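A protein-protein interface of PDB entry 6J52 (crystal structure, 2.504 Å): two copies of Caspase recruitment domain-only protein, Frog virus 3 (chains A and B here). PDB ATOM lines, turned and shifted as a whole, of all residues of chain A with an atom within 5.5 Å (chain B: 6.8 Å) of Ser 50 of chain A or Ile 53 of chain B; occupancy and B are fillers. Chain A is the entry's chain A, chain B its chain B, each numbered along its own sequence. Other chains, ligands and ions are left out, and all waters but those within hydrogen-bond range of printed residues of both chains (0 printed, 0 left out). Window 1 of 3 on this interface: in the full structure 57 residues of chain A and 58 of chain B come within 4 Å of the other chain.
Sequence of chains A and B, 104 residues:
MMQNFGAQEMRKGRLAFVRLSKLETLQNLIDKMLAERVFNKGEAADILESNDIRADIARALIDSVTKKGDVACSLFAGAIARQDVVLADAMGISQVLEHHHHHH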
ATOM      1  N   ASP A  46     -21.804  15.713  26.636  1.00  0.00           N
ATOM      2  CA  ASP A  46     -22.855  15.140  25.794  1.00  0.00           C
ATOM      3  C   ASP A  46     -24.186  15.869  25.965  1.00  0.00           C
ATOM      4  O   ASP A  46     -24.864  16.189  24.977  1.00  0.00           O
ATOM      5  CB  ASP A  46     -23.017  13.654  26.118  1.00  0.00           C
ATOM      6  CG  ASP A  46     -23.896  12.929  25.113  1.00  0.00           C
ATOM      7  OD1 ASP A  46     -23.487  12.798  23.937  1.00  0.00           O
ATOM      8  OD2 ASP A  46     -24.999  12.486  25.501  1.00  0.00           O
ATOM      9  N   ILE A  47     -24.596  16.113  27.217  1.00  0.00           N
ATOM     10  CA  ILE A  47     -25.872  16.777  27.456  1.00  0.00           C
ATOM     11  C   ILE A  47     -25.872  18.167  26.844  1.00  0.00           C
ATOM     12  O   ILE A  47     -26.866  18.604  26.255  1.00  0.00           O
ATOM     13  CB  ILE A  47     -26.174  16.820  28.960  1.00  0.00           C
ATOM     14  CG1 ILE A  47     -26.488  15.406  29.450  1.00  0.00           C
ATOM     15  CG2 ILE A  47     -27.312  17.790  29.248  1.00  0.00           C
ATOM     16  CD1 ILE A  47     -26.205  15.199  30.924  1.00  0.00           C
ATOM     17  N   LEU A  48     -24.750  18.871  26.952  1.00  0.00           N
ATOM     18  CA  LEU A  48     -24.653  20.223  26.432  1.00  0.00           C
ATOM     19  C   LEU A  48     -24.549  20.256  24.923  1.00  0.00           C
ATOM     20  O   LEU A  48     -24.975  21.231  24.298  1.00  0.00           O
ATOM     21  CB  LEU A  48     -23.441  20.920  27.026  1.00  0.00           C
ATOM     22  CG  LEU A  48     -23.746  21.397  28.428  1.00  0.00           C
ATOM     23  CD1 LEU A  48     -22.459  21.891  29.077  1.00  0.00           C
ATOM     24  CD2 LEU A  48     -24.818  22.486  28.320  1.00  0.00           C
ATOM     25  N   GLU A  49     -23.974  19.227  24.325  1.00  0.00           N
ATOM     26  CA  GLU A  49     -23.751  19.252  22.891  1.00  0.00           C
ATOM     27  C   GLU A  49     -25.077  19.085  22.160  1.00  0.00           C
ATOM     28  O   GLU A  49     -25.848  18.163  22.446  1.00  0.00           O
ATOM     29  CB  GLU A  49     -22.758  18.164  22.484  1.00  0.00           C
ATOM     30  CG  GLU A  49     -22.485  18.125  20.992  1.00  0.00           C
ATOM     31  CD  GLU A  49     -23.486  17.257  20.251  1.00  0.00           C
ATOM     32  OE1 GLU A  49     -23.884  16.204  20.805  1.00  0.00           O
ATOM     33  OE2 GLU A  49     -23.883  17.633  19.130  1.00  0.00           O
ATOM     34  N   SER A  50     -25.337  19.994  21.227  1.00  0.00           N
ATOM     35  CA  SER A  50     -26.523  19.950  20.376  1.00  0.00           C
ATOM     36  C   SER A  50     -26.156  20.530  19.005  1.00  0.00           C
ATOM     37  O   SER A  50     -26.831  21.414  18.469  1.00  0.00           O
ATOM     38  CB  SER A  50     -27.689  20.687  21.038  1.00  0.00           C
ATOM     39  OG  SER A  50     -27.221  21.798  21.785  1.00  0.00           O
ATOM     40  N   ASN A  51     -25.054  20.024  18.436  1.00  0.00           N
ATOM     41  CA  ASN A  51     -24.557  20.505  17.154  1.00  0.00           C
ATOM     42  C   ASN A  51     -25.527  20.211  16.021  1.00  0.00           C
ATOM     43  O   ASN A  51     -25.630  21.009  15.082  1.00  0.00           O
ATOM     44  CB  ASN A  51     -23.197  19.877  16.848  1.00  0.00           C
ATOM     45  CG  ASN A  51     -22.626  20.338  15.505  1.00  0.00           C
ATOM     46  OD1 ASN A  51     -22.273  21.509  15.346  1.00  0.00           O
ATOM     47  ND2 ASN A  51     -22.522  19.411  14.538  1.00  0.00           N
ATOM     48  N   ASP A  52     -26.241  19.082  16.079  1.00  0.00           N
ATOM     49  CA  ASP A  52     -27.172  18.766  15.001  1.00  0.00           C
ATOM     50  C   ASP A  52     -28.289  19.803  14.901  1.00  0.00           C
ATOM     51  O   ASP A  52     -28.638  20.239  13.801  1.00  0.00           O
ATOM     52  CB  ASP A  52     -27.743  17.362  15.184  1.00  0.00           C
ATOM     53  CG  ASP A  52     -26.679  16.295  15.130  1.00  0.00           C
ATOM     54  OD1 ASP A  52     -25.648  16.527  14.463  1.00  0.00           O
ATOM     55  OD2 ASP A  52     -26.888  15.201  15.708  1.00  0.00           O
ATOM     56  N   ILE A  53     -28.857  20.218  16.032  1.00  0.00           N
ATOM     57  CA  ILE A  53     -29.870  21.265  15.981  1.00  0.00           C
ATOM     58  C   ILE A  53     -29.239  22.598  15.600  1.00  0.00           C
ATOM     59  O   ILE A  53     -29.815  23.370  14.824  1.00  0.00           O
ATOM     60  CB  ILE A  53     -30.631  21.354  17.312  1.00  0.00           C
ATOM     61  CG1 ILE A  53     -31.349  20.038  17.605  1.00  0.00           C
ATOM     62  CG2 ILE A  53     -31.660  22.461  17.254  1.00  0.00           C
ATOM     63  CD1 ILE A  53     -32.124  20.069  18.892  1.00  0.00           C
ATOM     64  N   ARG A  54     -28.039  22.875  16.115  1.00  0.00           N
ATOM     65  CA  ARG A  54     -27.319  24.088  15.741  1.00  0.00           C
ATOM     66  C   ARG A  54     -27.173  24.197  14.225  1.00  0.00           C
ATOM     67  O   ARG A  54     -27.589  25.189  13.608  1.00  0.00           O
ATOM     68  CB  ARG A  54     -25.940  24.104  16.412  1.00  0.00           C
ATOM     69  CG  ARG A  54     -25.271  25.478  16.396  1.00  0.00           C
ATOM     70  CD  ARG A  54     -23.765  25.354  16.356  1.00  0.00           C
ATOM     71  NE  ARG A  54     -23.323  24.338  15.399  1.00  0.00           N
ATOM     72  CZ  ARG A  54     -23.166  24.564  14.098  1.00  0.00           C
ATOM     73  NH1 ARG A  54     -23.401  25.779  13.591  1.00  0.00           N
ATOM     74  NH2 ARG A  54     -22.781  23.576  13.303  1.00  0.00           N
ATOM     75  N   ALA A  55     -26.586  23.169  13.610  1.00  0.00           N
ATOM     76  CA  ALA A  55     -26.409  23.164  12.163  1.00  0.00           C
ATOM     77  C   ALA A  55     -27.744  23.287  11.441  1.00  0.00           C
ATOM     78  O   ALA A  55     -27.822  23.912  10.381  1.00  0.00           O
ATOM     79  CB  ALA A  55     -25.664  21.896  11.721  1.00  0.00           C
ATOM     80  N   ILE A  57     -30.389  24.960  12.570  1.00  0.00           N
ATOM     81  CA  ILE A  57     -30.688  26.391  12.643  1.00  0.00           C
ATOM     82  C   ILE A  57     -29.911  27.158  11.575  1.00  0.00           C
ATOM     83  O   ILE A  57     -30.443  28.076  10.942  1.00  0.00           O
ATOM     84  CB  ILE A  57     -30.380  26.944  14.049  1.00  0.00           C
ATOM     85  CG1 ILE A  57     -31.268  26.307  15.116  1.00  0.00           C
ATOM     86  CG2 ILE A  57     -30.523  28.449  14.079  1.00  0.00           C
ATOM     87  CD1 ILE A  57     -30.986  26.813  16.480  1.00  0.00           C
ATOM     88  N   LEU B  23     -23.632  29.244  18.257  1.00  0.00           N
ATOM     89  CA  LEU B  23     -25.070  29.377  18.470  1.00  0.00           C
ATOM     90  C   LEU B  23     -25.445  30.816  18.801  1.00  0.00           C
ATOM     91  O   LEU B  23     -26.497  31.305  18.374  1.00  0.00           O
ATOM     92  CB  LEU B  23     -25.529  28.428  19.577  1.00  0.00           C
ATOM     93  CG  LEU B  23     -27.022  28.528  19.906  1.00  0.00           C
ATOM     94  CD1 LEU B  23     -27.834  28.038  18.707  1.00  0.00           C
ATOM     95  CD2 LEU B  23     -27.383  27.766  21.186  1.00  0.00           C
ATOM     96  N   GLN B  27     -28.212  33.333  16.862  1.00  0.00           N
ATOM     97  CA  GLN B  27     -29.324  34.054  17.481  1.00  0.00           C
ATOM     98  C   GLN B  27     -29.191  35.562  17.281  1.00  0.00           C
ATOM     99  O   GLN B  27     -30.191  36.258  17.053  1.00  0.00           O
ATOM    100  CB  GLN B  27     -29.403  33.705  18.965  1.00  0.00           C
ATOM    101  CG  GLN B  27     -29.498  32.208  19.202  1.00  0.00           C
ATOM    102  CD  GLN B  27     -29.160  31.818  20.631  1.00  0.00           C
ATOM    103  OE1 GLN B  27     -28.276  32.404  21.257  1.00  0.00           O
ATOM    104  NE2 GLN B  27     -29.874  30.828  21.158  1.00  0.00           N
ATOM    105  N   LEU B  48     -36.616  29.210  14.680  1.00  0.00           N
ATOM    106  CA  LEU B  48     -36.267  28.869  16.054  1.00  0.00           C
ATOM    107  C   LEU B  48     -37.189  27.811  16.648  1.00  0.00           C
ATOM    108  O   LEU B  48     -36.724  26.922  17.367  1.00  0.00           O
ATOM    109  CB  LEU B  48     -36.279  30.129  16.911  1.00  0.00           C
ATOM    110  CG  LEU B  48     -35.105  31.042  16.579  1.00  0.00           C
ATOM    111  CD1 LEU B  48     -35.352  32.467  17.076  1.00  0.00           C
ATOM    112  CD2 LEU B  48     -33.817  30.434  17.169  1.00  0.00           C
ATOM    113  N   ASN B  51     -36.490  24.191  15.994  1.00  0.00           N
ATOM    114  CA  ASN B  51     -35.161  23.751  16.384  1.00  0.00           C
ATOM    115  C   ASN B  51     -34.846  24.248  17.807  1.00  0.00           C
ATOM    116  O   ASN B  51     -34.026  25.129  18.033  1.00  0.00           O
ATOM    117  CB  ASN B  51     -34.122  24.263  15.376  1.00  0.00           C
ATOM    118  CG  ASN B  51     -34.466  23.906  13.917  1.00  0.00           C
ATOM    119  OD1 ASN B  51     -34.592  22.735  13.571  1.00  0.00           O
ATOM    120  ND2 ASN B  51     -34.606  24.920  13.064  1.00  0.00           N
ATOM    121  N   ASP B  52     -35.513  23.686  18.810  1.00  0.00           N
ATOM    122  CA  ASP B  52     -35.344  24.145  20.187  1.00  0.00           C
ATOM    123  C   ASP B  52     -34.172  23.386  20.806  1.00  0.00           C
ATOM    124  O   ASP B  52     -34.293  22.216  21.177  1.00  0.00           O
ATOM    125  CB  ASP B  52     -36.650  23.951  20.955  1.00  0.00           C
ATOM    126  CG  ASP B  52     -36.731  24.776  22.251  1.00  0.00           C
ATOM    127  OD1 ASP B  52     -37.814  24.768  22.892  1.00  0.00           O
ATOM    128  OD2 ASP B  52     -35.718  25.389  22.653  1.00  0.00           O
ATOM    129  N   ILE B  53     -33.021  24.063  20.899  1.00  0.00           N
ATOM    130  CA  ILE B  53     -31.861  23.494  21.584  1.00  0.00           C
ATOM    131  C   ILE B  53     -32.133  23.361  23.084  1.00  0.00           C
ATOM    132  O   ILE B  53     -31.723  22.385  23.722  1.00  0.00           O
ATOM    133  CB  ILE B  53     -30.608  24.351  21.313  1.00  0.00           C
ATOM    134  CG1 ILE B  53     -30.028  24.034  19.943  1.00  0.00           C
ATOM    135  CG2 ILE B  53     -29.534  24.114  22.384  1.00  0.00           C
ATOM    136  CD1 ILE B  53     -28.652  24.636  19.674  1.00  0.00           C
ATOM    137  N   ARG B  54     -32.837  24.338  23.664  1.00  0.00           N
ATOM    138  CA  ARG B  54     -33.096  24.324  25.097  1.00  0.00           C
ATOM    139  C   ARG B  54     -33.892  23.089  25.492  1.00  0.00           C
ATOM    140  O   ARG B  54     -33.518  22.366  26.420  1.00  0.00           O
ATOM    141  CB  ARG B  54     -33.829  25.602  25.506  1.00  0.00           C
ATOM    142  CG  ARG B  54     -34.025  25.748  27.006  1.00  0.00           C
ATOM    143  CD  ARG B  54     -35.333  26.462  27.343  1.00  0.00           C
ATOM    144  NE  ARG B  54     -36.467  25.892  26.631  1.00  0.00           N
ATOM    145  CZ  ARG B  54     -37.199  24.881  27.087  1.00  0.00           C
ATOM    146  NH1 ARG B  54     -36.909  24.327  28.260  1.00  0.00           N
ATOM    147  NH2 ARG B  54     -38.220  24.423  26.375  1.00  0.00           N
ATOM    148  N   ALA B  55     -34.981  22.817  24.774  1.00  0.00           N
ATOM    149  CA  ALA B  55     -35.780  21.637  25.071  1.00  0.00           C
ATOM    150  C   ALA B  55     -34.963  20.356  24.917  1.00  0.00           C
ATOM    151  O   ALA B  55     -35.127  19.409  25.697  1.00  0.00           O
ATOM    152  CB  ALA B  55     -37.013  21.608  24.174  1.00  0.00           C
ATOM    153  N   ASP B  56     -34.081  20.311  23.912  1.00  0.00           N
ATOM    154  CA  ASP B  56     -33.228  19.142  23.702  1.00  0.00           C
ATOM    155  C   ASP B  56     -32.287  18.931  24.882  1.00  0.00           C
ATOM    156  O   ASP B  56     -32.136  17.806  25.380  1.00  0.00           O
ATOM    157  CB  ASP B  56     -32.430  19.311  22.419  1.00  0.00           C
ATOM    158  CG  ASP B  56     -31.743  18.020  21.973  1.00  0.00           C
ATOM    159  OD1 ASP B  56     -32.453  17.091  21.529  1.00  0.00           O
ATOM    160  OD2 ASP B  56     -30.495  17.938  22.058  1.00  0.00           O
ATOM    161  N   ILE B  57     -31.646  20.010  25.343  1.00  0.00           N
ATOM    162  CA  ILE B  57     -30.752  19.918  26.492  1.00  0.00           C
ATOM    163  C   ILE B  57     -31.519  19.500  27.747  1.00  0.00           C
ATOM    164  O   ILE B  57     -31.019  18.713  28.553  1.00  0.00           O
ATOM    165  CB  ILE B  57     -30.015  21.250  26.703  1.00  0.00           C
ATOM    166  CG1 ILE B  57     -29.144  21.574  25.497  1.00  0.00           C
ATOM    167  CG2 ILE B  57     -29.167  21.190  27.956  1.00  0.00           C
ATOM    168  CD1 ILE B  57     -28.371  22.848  25.652  1.00  0.00           C
ATOM    169  N   ALA B  58     -32.739  20.013  27.927  1.00  0.00           N
ATOM    170  CA  ALA B  58     -33.511  19.701  29.129  1.00  0.00           C
ATOM    171  C   ALA B  58     -33.882  18.221  29.186  1.00  0.00           C
ATOM    172  O   ALA B  58     -33.801  17.595  30.253  1.00  0.00           O
ATOM    173  CB  ALA B  58     -34.765  20.586  29.195  1.00  0.00           C
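Leu 48 of chain A touches Ile 57 of chain B, but with the chains exchanged Ile 57 of chain A does not touch Leu 48 of chain B (4.6 Å). Ile 53 of chain A touches Asn 51 of chain B, but with the chains exchanged Asn 51 of chain A does not touch Ile 53 of chain B (6.0 Å). Ile 53 of chain A touches Asp 52 of chain B, but with the chains exchanged Asp 52 of chain A does not touch Ile 53 of chain B (6.8 Å). Ile 57 of chain A touches Asn 51 of chain B, but with the chains exchanged Asn 51 of chain A does not touch Ile 57 of chain B (8.3 Å). 7 positions are printed for both chains. Of the 8 pairs that touch across the chains among the printed residues, 1 has its exchanged pair printed and touching as well.
The side-chain carboxylate of Asp 52 of chain B is in salt-bridge range of the guanidinium group of Arg 54 of chain B, at 3.5 Å. The side-chain carboxylate (OD2) of Asp 52 of chain B is in hydrogen-bond range of the backbone NH (N) of Ala 55 of chain B (3.4 Å). The backbone carbonyl oxygen (O) of Leu 48 of chain A is in hydrogen-bond range of the side-chain hydroxyl (OG) of Ser 50 of chain A.
Ser 50 of chain A touches just one residue of chain B: Ile 53 (3.3 Å). Of the printed residues of chain A, Ile 53 of chain B touches Ser 50 (3.3 Å) and Ile 53 (3.5 Å). Of the printed residues of chain B, Ile 47 of chain A touches Ile 57 (3.8 Å). Printed residues of chain B within 4 Å of Leu 48 of chain A: Ile 57. Of the printed residues of chain A, Ile 57 of chain B touches Ile 47 and Leu 48. Of the printed residues of chain A, Asn 51 of chain B touches Ile 53 (3.6 Å) and Ile 57 (3.5 Å). Printed residues of chain A within 4 Å of Asp 56 of chain B: Ile 53. The nearest residue of chain B that does not touch Ser 50 of chain A is Asp 56 of chain B (4.1 Å). The nearest printed residue of chain A that does not touch Ile 53 of chain B is Arg 54 of chain A (4.02 Å). The nearest printed residue of chain B that does not touch Ile 47 of chain A is Asp 56 of chain B (5.4 Å).
Printed residues of chain B that touch a printed residue of chain A: Asn 51, Asp 52, Ile 53, Asp 56 and Ile 57. Hydrophobic or aromatic side chains of chain B that line the printed part of chain A: Ile 53 and Ile 57. Of the 11 printed residues of chain A, 5 touch a printed residue of chain B. Among the printed residues, 8 pairs touch across the chains.
Among the printed residues, merely in contact across the chains: Ile 47 of chain A with Ile 57 of chain B, Leu 48 of chain A with Ile 57 of chain B, Ser 50 of chain A with Ile 53 of chain B, Ile 53 of chain A with Asn 51 of chain B, Ile 53 of chain A with Asp 52 of chain B, Ile 53 of chain A with Ile 53 of chain B, Ile 53 of chain A with Asp 56 of chain B and Ile 57 of chain A with Asn 51 of chain B.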
